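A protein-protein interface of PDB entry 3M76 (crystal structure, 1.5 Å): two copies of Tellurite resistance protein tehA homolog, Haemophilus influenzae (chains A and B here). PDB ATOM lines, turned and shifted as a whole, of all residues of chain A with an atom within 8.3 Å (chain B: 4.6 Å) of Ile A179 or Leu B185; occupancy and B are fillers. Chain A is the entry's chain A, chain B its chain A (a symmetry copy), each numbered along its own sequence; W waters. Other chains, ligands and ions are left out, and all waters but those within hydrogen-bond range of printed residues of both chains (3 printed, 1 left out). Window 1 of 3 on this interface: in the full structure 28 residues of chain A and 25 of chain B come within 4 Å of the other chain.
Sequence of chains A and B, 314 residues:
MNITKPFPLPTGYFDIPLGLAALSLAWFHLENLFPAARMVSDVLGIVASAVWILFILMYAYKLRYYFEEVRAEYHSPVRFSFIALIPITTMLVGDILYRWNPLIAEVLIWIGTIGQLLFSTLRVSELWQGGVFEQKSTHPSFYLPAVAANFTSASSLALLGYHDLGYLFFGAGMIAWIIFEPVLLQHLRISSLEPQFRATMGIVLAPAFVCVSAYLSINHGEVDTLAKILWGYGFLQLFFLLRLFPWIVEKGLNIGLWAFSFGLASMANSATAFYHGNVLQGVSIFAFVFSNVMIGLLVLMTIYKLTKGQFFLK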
ATOM      1  N   VAL A 124     -25.229   3.079  -0.269  1.00  0.00           N
ATOM      2  CA  VAL A 124     -24.000   3.685   0.233  1.00  0.00           C
ATOM      3  C   VAL A 124     -23.367   2.755   1.260  1.00  0.00           C
ATOM      4  O   VAL A 124     -22.162   2.533   1.231  1.00  0.00           O
ATOM      5  CB  VAL A 124     -24.213   5.106   0.764  1.00  0.00           C
ATOM      6  CG1 VAL A 124     -22.937   5.625   1.427  1.00  0.00           C
ATOM      7  CG2 VAL A 124     -24.671   6.008  -0.353  1.00  0.00           C
ATOM      8  N   LEU A 127     -21.457  -0.433  -0.006  1.00  0.00           N
ATOM      9  CA  LEU A 127     -20.088  -0.248  -0.444  1.00  0.00           C
ATOM     10  C   LEU A 127     -19.092  -0.707   0.609  1.00  0.00           C
ATOM     11  O   LEU A 127     -17.982  -1.148   0.265  1.00  0.00           O
ATOM     12  CB  LEU A 127     -19.824   1.207  -0.856  1.00  0.00           C
ATOM     13  CG  LEU A 127     -20.683   1.782  -1.976  1.00  0.00           C
ATOM     14  CD1 LEU A 127     -20.419   3.260  -2.128  1.00  0.00           C
ATOM     15  CD2 LEU A 127     -20.428   1.058  -3.291  1.00  0.00           C
ATOM     16  N   TRP A 128     -19.437  -0.564   1.894  1.00  0.00           N
ATOM     17  CA  TRP A 128     -18.545  -0.915   2.980  1.00  0.00           C
ATOM     18  C   TRP A 128     -18.275  -2.408   3.085  1.00  0.00           C
ATOM     19  O   TRP A 128     -17.420  -2.813   3.869  1.00  0.00           O
ATOM     20  CB  TRP A 128     -19.078  -0.424   4.331  1.00  0.00           C
ATOM     21  CG  TRP A 128     -19.226   1.008   4.555  1.00  0.00           C
ATOM     22  CD1 TRP A 128     -19.008   2.032   3.696  1.00  0.00           C
ATOM     23  CD2 TRP A 128     -19.744   1.600   5.746  1.00  0.00           C
ATOM     24  NE1 TRP A 128     -19.320   3.244   4.294  1.00  0.00           N
ATOM     25  CE2 TRP A 128     -19.802   2.992   5.548  1.00  0.00           C
ATOM     26  CE3 TRP A 128     -20.188   1.083   6.957  1.00  0.00           C
ATOM     27  CZ2 TRP A 128     -20.258   3.860   6.527  1.00  0.00           C
ATOM     28  CZ3 TRP A 128     -20.661   1.957   7.917  1.00  0.00           C
ATOM     29  CH2 TRP A 128     -20.693   3.318   7.698  1.00  0.00           C
ATOM     30  N   GLN A 129     -18.962  -3.238   2.288  1.00  0.00           N
ATOM     31  CA  GLN A 129     -18.668  -4.663   2.200  1.00  0.00           C
ATOM     32  C   GLN A 129     -17.389  -4.958   1.463  1.00  0.00           C
ATOM     33  O   GLN A 129     -16.863  -6.055   1.582  1.00  0.00           O
ATOM     34  CB  GLN A 129     -19.824  -5.443   1.570  1.00  0.00           C
ATOM     35  CG  GLN A 129     -21.103  -5.335   2.349  1.00  0.00           C
ATOM     36  CD  GLN A 129     -22.274  -6.021   1.676  1.00  0.00           C
ATOM     37  OE1 GLN A 129     -22.171  -6.478   0.532  1.00  0.00           O
ATOM     38  NE2 GLN A 129     -23.396  -6.080   2.364  1.00  0.00           N
ATOM     39  N   GLY A 130     -16.891  -3.991   0.710  1.00  0.00           N
ATOM     40  CA  GLY A 130     -15.643  -4.118   0.004  1.00  0.00           C
ATOM     41  C   GLY A 130     -15.695  -4.896  -1.287  1.00  0.00           C
ATOM     42  O   GLY A 130     -16.612  -5.622  -1.567  1.00  0.00           O
ATOM     43  N   PHE A 133     -16.474  -1.357  -5.069  1.00  0.00           N
ATOM     44  CA  PHE A 133     -15.887  -0.044  -5.195  1.00  0.00           C
ATOM     45  C   PHE A 133     -14.380  -0.229  -5.254  1.00  0.00           C
ATOM     46  O   PHE A 133     -13.803  -1.032  -4.511  1.00  0.00           O
ATOM     47  CB  PHE A 133     -16.294   0.741  -3.942  1.00  0.00           C
ATOM     48  CG  PHE A 133     -15.898   2.215  -3.915  1.00  0.00           C
ATOM     49  CD1 PHE A 133     -16.822   3.190  -4.208  1.00  0.00           C
ATOM     50  CD2 PHE A 133     -14.614   2.598  -3.521  1.00  0.00           C
ATOM     51  CE1 PHE A 133     -16.491   4.529  -4.122  1.00  0.00           C
ATOM     52  CE2 PHE A 133     -14.279   3.945  -3.478  1.00  0.00           C
ATOM     53  CZ  PHE A 133     -15.233   4.900  -3.742  1.00  0.00           C
ATOM     54  N   PHE A 142     -20.227  10.886  -5.938  1.00  0.00           N
ATOM     55  CA  PHE A 142     -20.576  10.296  -4.640  1.00  0.00           C
ATOM     56  C   PHE A 142     -21.181  11.335  -3.705  1.00  0.00           C
ATOM     57  O   PHE A 142     -21.980  10.980  -2.849  1.00  0.00           O
ATOM     58  CB  PHE A 142     -19.320   9.628  -4.038  1.00  0.00           C
ATOM     59  CG  PHE A 142     -19.534   8.961  -2.726  1.00  0.00           C
ATOM     60  CD1 PHE A 142     -19.873   7.631  -2.657  1.00  0.00           C
ATOM     61  CD2 PHE A 142     -19.355   9.660  -1.562  1.00  0.00           C
ATOM     62  CE1 PHE A 142     -20.031   7.000  -1.390  1.00  0.00           C
ATOM     63  CE2 PHE A 142     -19.532   9.068  -0.319  1.00  0.00           C
ATOM     64  CZ  PHE A 142     -19.843   7.707  -0.242  1.00  0.00           C
ATOM     65  N   TYR A 143     -20.863  12.616  -3.874  1.00  0.00           N
ATOM     66  CA  TYR A 143     -21.524  13.640  -3.070  1.00  0.00           C
ATOM     67  C   TYR A 143     -23.036  13.645  -3.197  1.00  0.00           C
ATOM     68  O   TYR A 143     -23.738  14.142  -2.315  1.00  0.00           O
ATOM     69  CB  TYR A 143     -21.049  15.035  -3.434  1.00  0.00           C
ATOM     70  CG  TYR A 143     -19.627  15.392  -3.053  1.00  0.00           C
ATOM     71  CD1 TYR A 143     -19.190  15.192  -1.791  1.00  0.00           C
ATOM     72  CD2 TYR A 143     -18.779  15.959  -3.972  1.00  0.00           C
ATOM     73  CE1 TYR A 143     -17.916  15.526  -1.419  1.00  0.00           C
ATOM     74  CE2 TYR A 143     -17.470  16.354  -3.621  1.00  0.00           C
ATOM     75  CZ  TYR A 143     -17.078  16.131  -2.320  1.00  0.00           C
ATOM     76  OH  TYR A 143     -15.776  16.480  -1.959  1.00  0.00           O
ATOM     77  N   VAL A 147     -24.268  13.399   0.485  1.00  0.00           N
ATOM     78  CA  VAL A 147     -24.191  14.750   1.004  1.00  0.00           C
ATOM     79  C   VAL A 147     -25.356  15.598   0.542  1.00  0.00           C
ATOM     80  O   VAL A 147     -26.160  16.083   1.357  1.00  0.00           O
ATOM     81  CB  VAL A 147     -22.827  15.392   0.614  1.00  0.00           C
ATOM     82  CG1 VAL A 147     -22.758  16.846   1.030  1.00  0.00           C
ATOM     83  CG2 VAL A 147     -21.693  14.603   1.240  1.00  0.00           C
ATOM     84  N   GLY A 171     -26.791  17.492   9.711  1.00  0.00           N
ATOM     85  CA  GLY A 171     -25.591  16.948  10.279  1.00  0.00           C
ATOM     86  C   GLY A 171     -25.084  15.719   9.560  1.00  0.00           C
ATOM     87  O   GLY A 171     -23.864  15.521   9.366  1.00  0.00           O
ATOM     88  N   ALA A 172     -25.997  14.862   9.134  1.00  0.00           N
ATOM     89  CA  ALA A 172     -25.641  13.694   8.331  1.00  0.00           C
ATOM     90  C   ALA A 172     -24.911  14.147   7.072  1.00  0.00           C
ATOM     91  O   ALA A 172     -23.854  13.615   6.728  1.00  0.00           O
ATOM     92  CB  ALA A 172     -26.871  12.901   7.994  1.00  0.00           C
ATOM     93  N   GLY A 173     -25.452  15.153   6.385  1.00  0.00           N
ATOM     94  CA  GLY A 173     -24.774  15.622   5.190  1.00  0.00           C
ATOM     95  C   GLY A 173     -23.449  16.321   5.432  1.00  0.00           C
ATOM     96  O   GLY A 173     -22.501  16.128   4.675  1.00  0.00           O
ATOM     97  N   MET A 174     -23.395  17.147   6.476  1.00  0.00           N
ATOM     98  CA  MET A 174     -22.201  17.927   6.699  1.00  0.00           C
ATOM     99  C   MET A 174     -21.016  17.037   7.096  1.00  0.00           C
ATOM    100  O   MET A 174     -19.893  17.159   6.597  1.00  0.00           O
ATOM    101  CB  MET A 174     -22.435  18.994   7.757  1.00  0.00           C
ATOM    102  CG  MET A 174     -21.223  19.890   7.946  1.00  0.00           C
ATOM    103  SD  MET A 174     -21.533  21.168   9.166  1.00  0.00           S
ATOM    104  CE  MET A 174     -19.908  21.887   9.262  1.00  0.00           C
ATOM    105  N   ILE A 175     -21.273  16.101   8.011  1.00  0.00           N
ATOM    106  CA  ILE A 175     -20.209  15.229   8.440  1.00  0.00           C
ATOM    107  C   ILE A 175     -19.873  14.244   7.300  1.00  0.00           C
ATOM    108  O   ILE A 175     -18.698  13.960   7.074  1.00  0.00           O
ATOM    109  CB  ILE A 175     -20.502  14.571   9.805  1.00  0.00           C
ATOM    110  CG1 ILE A 175     -20.603  15.664  10.871  1.00  0.00           C
ATOM    111  CG2 ILE A 175     -19.449  13.513  10.148  1.00  0.00           C
ATOM    112  CD1 ILE A 175     -21.040  15.210  12.206  1.00  0.00           C
ATOM    113  N   ALA A 176     -20.859  13.729   6.569  1.00  0.00           N
ATOM    114  CA  ALA A 176     -20.547  12.895   5.430  1.00  0.00           C
ATOM    115  C   ALA A 176     -19.644  13.594   4.407  1.00  0.00           C
ATOM    116  O   ALA A 176     -18.761  12.965   3.817  1.00  0.00           O
ATOM    117  CB  ALA A 176     -21.794  12.389   4.752  1.00  0.00           C
ATOM    118  N   TRP A 177     -19.869  14.880   4.213  1.00  0.00           N
ATOM    119  CA  TRP A 177     -19.062  15.682   3.295  1.00  0.00           C
ATOM    120  C   TRP A 177     -17.601  15.723   3.753  1.00  0.00           C
ATOM    121  O   TRP A 177     -16.673  15.387   2.979  1.00  0.00           O
ATOM    122  CB  TRP A 177     -19.638  17.089   3.221  1.00  0.00           C
ATOM    123  CG  TRP A 177     -18.715  18.120   2.636  1.00  0.00           C
ATOM    124  CD1 TRP A 177     -17.819  17.954   1.618  1.00  0.00           C
ATOM    125  CD2 TRP A 177     -18.635  19.489   3.019  1.00  0.00           C
ATOM    126  NE1 TRP A 177     -17.150  19.130   1.386  1.00  0.00           N
ATOM    127  CE2 TRP A 177     -17.632  20.093   2.236  1.00  0.00           C
ATOM    128  CE3 TRP A 177     -19.294  20.263   3.978  1.00  0.00           C
ATOM    129  CZ2 TRP A 177     -17.280  21.422   2.383  1.00  0.00           C
ATOM    130  CZ3 TRP A 177     -18.931  21.583   4.111  1.00  0.00           C
ATOM    131  CH2 TRP A 177     -17.950  22.139   3.323  1.00  0.00           C
ATOM    132  N   ILE A 178     -17.399  16.117   4.992  1.00  0.00           N
ATOM    133  CA  ILE A 178     -16.071  16.227   5.560  1.00  0.00           C
ATOM    134  C   ILE A 178     -15.349  14.880   5.547  1.00  0.00           C
ATOM    135  O   ILE A 178     -14.105  14.815   5.493  1.00  0.00           O
ATOM    136  CB  ILE A 178     -16.164  16.804   6.989  1.00  0.00           C
ATOM    137  CG1 ILE A 178     -16.672  18.241   6.891  1.00  0.00           C
ATOM    138  CG2 ILE A 178     -14.820  16.718   7.728  1.00  0.00           C
ATOM    139  CD1 ILE A 178     -15.905  19.154   5.923  1.00  0.00           C
ATOM    140  N   ILE A 179     -16.124  13.801   5.678  1.00  0.00           N
ATOM    141  CA  ILE A 179     -15.566  12.470   5.728  1.00  0.00           C
ATOM    142  C   ILE A 179     -15.185  11.927   4.342  1.00  0.00           C
ATOM    143  O   ILE A 179     -14.254  11.125   4.242  1.00  0.00           O
ATOM    144  CB  ILE A 179     -16.488  11.476   6.497  1.00  0.00           C
ATOM    145  CG1 ILE A 179     -16.725  11.909   7.961  1.00  0.00           C
ATOM    146  CG2 ILE A 179     -15.923  10.097   6.477  1.00  0.00           C
ATOM    147  CD1 ILE A 179     -15.586  12.335   8.659  1.00  0.00           C
ATOM    148  N   PHE A 180     -15.871  12.347   3.275  1.00  0.00           N
ATOM    149  CA  PHE A 180     -15.554  11.933   1.919  1.00  0.00           C
ATOM    150  C   PHE A 180     -14.513  12.785   1.212  1.00  0.00           C
ATOM    151  O   PHE A 180     -13.596  12.278   0.550  1.00  0.00           O
ATOM    152  CB  PHE A 180     -16.802  11.811   1.058  1.00  0.00           C
ATOM    153  CG  PHE A 180     -16.508  11.289  -0.327  1.00  0.00           C
ATOM    154  CD1 PHE A 180     -16.070  10.005  -0.464  1.00  0.00           C
ATOM    155  CD2 PHE A 180     -16.639  12.098  -1.447  1.00  0.00           C
ATOM    156  CE1 PHE A 180     -15.820   9.474  -1.714  1.00  0.00           C
ATOM    157  CE2 PHE A 180     -16.386  11.533  -2.732  1.00  0.00           C
ATOM    158  CZ  PHE A 180     -15.958  10.272  -2.813  1.00  0.00           C
ATOM    159  N   GLU A 181     -14.679  14.096   1.316  1.00  0.00           N
ATOM    160  CA  GLU A 181     -13.826  14.977   0.541  1.00  0.00           C
ATOM    161  C   GLU A 181     -12.308  14.707   0.670  1.00  0.00           C
ATOM    162  O   GLU A 181     -11.576  14.832  -0.320  1.00  0.00           O
ATOM    163  CB  GLU A 181     -14.176  16.443   0.760  1.00  0.00           C
ATOM    164  CG  GLU A 181     -13.409  17.404  -0.170  1.00  0.00           C
ATOM    165  CD  GLU A 181     -14.138  18.691  -0.435  1.00  0.00           C
ATOM    166  OE1 GLU A 181     -13.498  19.750  -0.348  1.00  0.00           O
ATOM    167  OE2 GLU A 181     -15.333  18.655  -0.811  1.00  0.00           O
ATOM    168  N   PRO A 182     -11.809  14.363   1.873  1.00  0.00           N
ATOM    169  CA  PRO A 182     -10.357  14.130   1.949  1.00  0.00           C
ATOM    170  C   PRO A 182      -9.850  13.105   0.943  1.00  0.00           C
ATOM    171  O   PRO A 182      -8.787  13.308   0.326  1.00  0.00           O
ATOM    172  CB  PRO A 182     -10.155  13.658   3.378  1.00  0.00           C
ATOM    173  CG  PRO A 182     -11.321  14.296   4.141  1.00  0.00           C
ATOM    174  CD  PRO A 182     -12.463  14.214   3.190  1.00  0.00           C
ATOM    175  N   VAL A 183     -10.542  11.990   0.825  1.00  0.00           N
ATOM    176  CA  VAL A 183     -10.094  10.933  -0.050  1.00  0.00           C
ATOM    177  C   VAL A 183     -10.379  11.261  -1.519  1.00  0.00           C
ATOM    178  O   VAL A 183      -9.624  10.838  -2.408  1.00  0.00           O
ATOM    179  CB  VAL A 183     -10.602   9.545   0.364  1.00  0.00           C
ATOM    180  CG1 VAL A 183     -10.106   9.217   1.785  1.00  0.00           C
ATOM    181  CG2 VAL A 183     -12.091   9.402   0.260  1.00  0.00           C
ATOM    182  N   LEU A 184     -11.416  12.054  -1.793  1.00  0.00           N
ATOM    183  CA  LEU A 184     -11.665  12.492  -3.135  1.00  0.00           C
ATOM    184  C   LEU A 184     -10.527  13.384  -3.634  1.00  0.00           C
ATOM    185  O   LEU A 184     -10.006  13.174  -4.736  1.00  0.00           O
ATOM    186  CB  LEU A 184     -12.986  13.246  -3.243  1.00  0.00           C
ATOM    187  CG  LEU A 184     -13.275  13.847  -4.639  1.00  0.00           C
ATOM    188  CD1 LEU A 184     -13.399  12.765  -5.708  1.00  0.00           C
ATOM    189  CD2 LEU A 184     -14.493  14.704  -4.590  1.00  0.00           C
ATOM    190  N   ILE B 178     -12.757  12.899  13.141  1.00  0.00           N
ATOM    191  CA  ILE B 178     -12.936  13.442  11.811  1.00  0.00           C
ATOM    192  C   ILE B 178     -11.715  13.174  10.932  1.00  0.00           C
ATOM    193  O   ILE B 178     -11.819  13.076   9.694  1.00  0.00           O
ATOM    194  CB  ILE B 178     -13.245  14.952  11.904  1.00  0.00           C
ATOM    195  CG1 ILE B 178     -14.601  15.121  12.586  1.00  0.00           C
ATOM    196  CG2 ILE B 178     -13.206  15.628  10.526  1.00  0.00           C
ATOM    197  CD1 ILE B 178     -15.756  14.309  11.983  1.00  0.00           C
ATOM    198  N   GLU B 181     -11.758   8.854  10.377  1.00  0.00           N
ATOM    199  CA  GLU B 181     -12.860   8.224   9.675  1.00  0.00           C
ATOM    200  C   GLU B 181     -12.767   8.263   8.131  1.00  0.00           C
ATOM    201  O   GLU B 181     -13.152   7.292   7.468  1.00  0.00           O
ATOM    202  CB  GLU B 181     -14.210   8.706  10.189  1.00  0.00           C
ATOM    203  CG  GLU B 181     -15.405   7.939   9.590  1.00  0.00           C
ATOM    204  CD  GLU B 181     -16.616   7.924  10.481  1.00  0.00           C
ATOM    205  OE1 GLU B 181     -17.717   8.179   9.970  1.00  0.00           O
ATOM    206  OE2 GLU B 181     -16.492   7.578  11.679  1.00  0.00           O
ATOM    207  N   PRO B 182     -12.290   9.374   7.536  1.00  0.00           N
ATOM    208  CA  PRO B 182     -12.234   9.370   6.065  1.00  0.00           C
ATOM    209  C   PRO B 182     -11.470   8.187   5.487  1.00  0.00           C
ATOM    210  O   PRO B 182     -11.908   7.587   4.487  1.00  0.00           O
ATOM    211  CB  PRO B 182     -11.556  10.687   5.739  1.00  0.00           C
ATOM    212  CG  PRO B 182     -11.898  11.582   6.936  1.00  0.00           C
ATOM    213  CD  PRO B 182     -11.836  10.661   8.104  1.00  0.00           C
ATOM    214  N   VAL B 183     -10.313   7.892   6.043  1.00  0.00           N
ATOM    215  CA  VAL B 183      -9.486   6.834   5.514  1.00  0.00           C
ATOM    216  C   VAL B 183     -10.021   5.453   5.907  1.00  0.00           C
ATOM    217  O   VAL B 183      -9.856   4.485   5.149  1.00  0.00           O
ATOM    218  CB  VAL B 183      -7.994   7.012   5.829  1.00  0.00           C
ATOM    219  CG1 VAL B 183      -7.495   8.339   5.229  1.00  0.00           C
ATOM    220  CG2 VAL B 183      -7.682   6.923   7.293  1.00  0.00           C
ATOM    221  N   LEU B 184     -10.710   5.350   7.043  1.00  0.00           N
ATOM    222  CA  LEU B 184     -11.336   4.113   7.409  1.00  0.00           C
ATOM    223  C   LEU B 184     -12.438   3.750   6.411  1.00  0.00           C
ATOM    224  O   LEU B 184     -12.488   2.613   5.923  1.00  0.00           O
ATOM    225  CB  LEU B 184     -11.922   4.175   8.814  1.00  0.00           C
ATOM    226  CG  LEU B 184     -12.711   2.913   9.241  1.00  0.00           C
ATOM    227  CD1 LEU B 184     -11.821   1.674   9.284  1.00  0.00           C
ATOM    228  CD2 LEU B 184     -13.385   3.144  10.550  1.00  0.00           C
ATOM    229  N   LEU B 185     -13.348   4.685   6.115  1.00  0.00           N
ATOM    230  CA  LEU B 185     -14.454   4.316   5.237  1.00  0.00           C
ATOM    231  C   LEU B 185     -14.001   4.037   3.810  1.00  0.00           C
ATOM    232  O   LEU B 185     -14.558   3.146   3.144  1.00  0.00           O
ATOM    233  CB  LEU B 185     -15.576   5.339   5.303  1.00  0.00           C
ATOM    234  CG  LEU B 185     -16.199   5.631   6.674  1.00  0.00           C
ATOM    235  CD1 LEU B 185     -17.432   6.526   6.529  1.00  0.00           C
ATOM    236  CD2 LEU B 185     -16.523   4.343   7.468  1.00  0.00           C
ATOM    237  N   GLN B 186     -12.983   4.751   3.350  1.00  0.00           N
ATOM    238  CA  GLN B 186     -12.427   4.452   2.050  1.00  0.00           C
ATOM    239  C   GLN B 186     -11.822   3.032   2.025  1.00  0.00           C
ATOM    240  O   GLN B 186     -12.000   2.300   1.045  1.00  0.00           O
ATOM    241  CB  GLN B 186     -11.392   5.497   1.648  1.00  0.00           C
ATOM    242  CG  GLN B 186     -10.763   5.293   0.288  1.00  0.00           C
ATOM    243  CD  GLN B 186     -11.625   5.710  -0.893  1.00  0.00           C
ATOM    244  OE1 GLN B 186     -12.860   5.904  -0.763  1.00  0.00           O
ATOM    245  NE2 GLN B 186     -10.998   5.803  -2.085  1.00  0.00           N
ATOM    246  N   HIS B 187     -11.129   2.660   3.088  1.00  0.00           N
ATOM    247  CA  HIS B 187     -10.582   1.320   3.193  1.00  0.00           C
ATOM    248  C   HIS B 187     -11.668   0.270   3.189  1.00  0.00           C
ATOM    249  O   HIS B 187     -11.529  -0.764   2.494  1.00  0.00           O
ATOM    250  CB  HIS B 187      -9.722   1.214   4.426  1.00  0.00           C
ATOM    251  CG  HIS B 187      -9.123  -0.136   4.616  1.00  0.00           C
ATOM    252  ND1 HIS B 187      -8.159  -0.640   3.767  1.00  0.00           N
ATOM    253  CD2 HIS B 187      -9.371  -1.092   5.536  1.00  0.00           C
ATOM    254  CE1 HIS B 187      -7.847  -1.869   4.166  1.00  0.00           C
ATOM    255  NE2 HIS B 187      -8.554  -2.163   5.246  1.00  0.00           N
ATOM    256  N   LEU B 188     -12.722   0.488   3.966  1.00  0.00           N
ATOM    257  CA  LEU B 188     -13.832  -0.476   3.990  1.00  0.00           C
ATOM    258  C   LEU B 188     -14.457  -0.624   2.608  1.00  0.00           C
ATOM    259  O   LEU B 188     -14.806  -1.730   2.196  1.00  0.00           O
ATOM    260  CB  LEU B 188     -14.886  -0.103   5.002  1.00  0.00           C
ATOM    261  CG  LEU B 188     -14.400  -0.105   6.436  1.00  0.00           C
ATOM    262  CD1 LEU B 188     -15.558   0.346   7.317  1.00  0.00           C
ATOM    263  CD2 LEU B 188     -13.918  -1.468   6.889  1.00  0.00           C
ATOM    264  N   ARG B 189     -14.602   0.491   1.887  1.00  0.00           N
ATOM    265  CA  ARG B 189     -15.184   0.428   0.563  1.00  0.00           C
ATOM    266  C   ARG B 189     -14.351  -0.452  -0.375  1.00  0.00           C
ATOM    267  O   ARG B 189     -14.883  -1.204  -1.211  1.00  0.00           O
ATOM    268  CB  ARG B 189     -15.325   1.819  -0.057  1.00  0.00           C
ATOM    269  CG  ARG B 189     -16.489   2.666   0.472  1.00  0.00           C
ATOM    270  CD  ARG B 189     -16.714   3.885  -0.386  1.00  0.00           C
ATOM    271  NE  ARG B 189     -15.727   4.936  -0.151  1.00  0.00           N
ATOM    272  CZ  ARG B 189     -15.849   5.872   0.786  1.00  0.00           C
ATOM    273  NH1 ARG B 189     -16.950   5.908   1.531  1.00  0.00           N
ATOM    274  NH2 ARG B 189     -14.883   6.770   0.957  1.00  0.00           N
ATOM    275  N   TYR B 233     -25.705  12.490  12.116  1.00  0.00           N
ATOM    276  CA  TYR B 233     -24.721  11.580  11.540  1.00  0.00           C
ATOM    277  C   TYR B 233     -24.724  10.252  12.274  1.00  0.00           C
ATOM    278  O   TYR B 233     -24.599   9.190  11.651  1.00  0.00           O
ATOM    279  CB  TYR B 233     -23.312  12.174  11.559  1.00  0.00           C
ATOM    280  CG  TYR B 233     -22.309  11.424  10.768  1.00  0.00           C
ATOM    281  CD1 TYR B 233     -22.319  11.474   9.387  1.00  0.00           C
ATOM    282  CD2 TYR B 233     -21.389  10.598  11.381  1.00  0.00           C
ATOM    283  CE1 TYR B 233     -21.387  10.782   8.643  1.00  0.00           C
ATOM    284  CE2 TYR B 233     -20.461   9.872  10.620  1.00  0.00           C
ATOM    285  CZ  TYR B 233     -20.480   9.986   9.248  1.00  0.00           C
ATOM    286  OH  TYR B 233     -19.530   9.312   8.476  1.00  0.00           O
ATOM    287  N   GLN B 237     -25.280   6.491  10.474  1.00  0.00           N
ATOM    288  CA  GLN B 237     -24.379   5.355  10.664  1.00  0.00           C
ATOM    289  C   GLN B 237     -25.124   4.150  11.230  1.00  0.00           C
ATOM    290  O   GLN B 237     -24.895   3.007  10.819  1.00  0.00           O
ATOM    291  CB  GLN B 237     -23.202   5.692  11.572  1.00  0.00           C
ATOM    292  CG  GLN B 237     -22.300   6.815  11.050  1.00  0.00           C
ATOM    293  CD  GLN B 237     -21.587   6.511   9.764  1.00  0.00           C
ATOM    294  OE1 GLN B 237     -22.199   6.442   8.698  1.00  0.00           O
ATOM    295  NE2 GLN B 237     -20.265   6.310   9.848  1.00  0.00           N
HETATM  296  O   HOH W   1     -19.721   6.394   3.432  1.00  0.00           O
HETATM  297  O   HOH W   2     -19.666   4.455   1.370  1.00  0.00           O
HETATM  298  O   HOH W   3     -14.313   8.480   3.305  1.00  0.00           O
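The side-chain carboxylate of Glu B181 sits at hydrogen-bond distance from the side-chain amide nitrogen of Gln B237 (3.2 Å).
The side-chain amide oxygen (OE1) of Gln B186 lies within hydrogen-bond range of the guanidinium group (NH2) of Arg B189 (2.8 Å).
The side-chain hydroxyl (OH) of Tyr B233 lies within hydrogen-bond range of the side-chain amide nitrogen (NE2) of Gln B237, 3.4 Å away.
Among the printed residues, pairs that only touch across the chains: Ile A179 with Pro B182, Gly A130 with Arg B189, Ile A178 with Ile B178, Ile A175 with Tyr B233, Trp A128 with Gln B237, Val A183 with Pro B182, Phe A133 with Gln B186, Ala A176 with Tyr B233, Val A183 with Gln B186, Phe A180 with Arg B189, Ala A172 with Tyr B233, Leu A127 with Leu B188, Ile A179 with Glu B181, Phe A142 with Arg B189, Ile A179 with Tyr B233, Ile A179 with Ile B178, Ile A179 with Leu B185, Trp A128 with Leu B185, Val A183 with Arg B189 and Pro A182 with Pro B182.
Water W3 lies within hydrogen-bond range of O of Ile A179 (2.8 Å), O of Pro B182 (2.8 Å) and NH2 of Arg B189 (3.0 Å).
Water W2 lies within hydrogen-bond range of the guanidinium group of Arg B189, the backbone carbonyl oxygen of Val A124 and the indole nitrogen of Trp A128.
Water W1 lies within hydrogen-bond range of the indole nitrogen (NE1) of Trp A128 and the guanidinium group (NH1) of Arg B189.
Ile A178 touches its own counterpart, Ile B178.
Pro A182 touches its own counterpart, Pro B182.
Val A183 touches Pro B182, but with the chains exchanged Pro A182 does not touch Val B183 (6.2 Å).
5 positions are printed for both chains.
Of the 24 pairs that touch across the chains among the printed residues, 2 have their exchanged pair printed and touching as well.
Printed residues of chain A that touch a printed residue of chain B: Leu A127, Trp A128, Gly A130, Phe A133, Phe A142, Ala A172, Ile A175, Ala A176, Ile A178, Ile A179, Phe A180, Pro A182 and Val A183.
Printed residues of chain B that touch a printed residue of chain A: Ile B178, Glu B181, Pro B182, Leu B185, Gln B186, Leu B188, Arg B189, Tyr B233 and Gln B237.
Hydrophobic or aromatic side chains of chain B within 4 Å of the printed part of chain A: Ile B178, Pro B182, Leu B185, Leu B188 and Tyr B233.
Along chain B the printed residues that touch a printed residue of chain A span positions 178 to 237.
Among the printed residues, 24 pairs touch across the chains.
The backbone carbonyl oxygen (O) of Leu B188 sits close to the backbone NH (N) of Gly A130.
The backbone carbonyl oxygen (O) of Leu A127 sits close to the backbone carbonyl oxygen (O) of Arg B189, 3.4 Å away.
O of Trp A128 lies close to O of Leu B188, 3.3 Å away.
O of Phe A133 sits close to O of Arg B189.
Printed residues of chain B within 4 Å of Ile A179: Ile B178, Glu B181, Pro B182, Leu B185 and Tyr B233.
Printed residues of chain A within 4 Å of Arg B189: Leu A127, Gly A130, Phe A133, Phe A142, Phe A180 and Val A183.
Of the printed residues of chain B, Phe A142 touches Arg B189.
Printed residues of chain A within 4 Å of Glu B181: Ile A179.
Of the printed residues of chain B, Ile A178 touches Ile B178 (3.4 Å).
The nearest printed residue of chain B that does not touch Ile A179 is Val B183 (5.4 Å).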
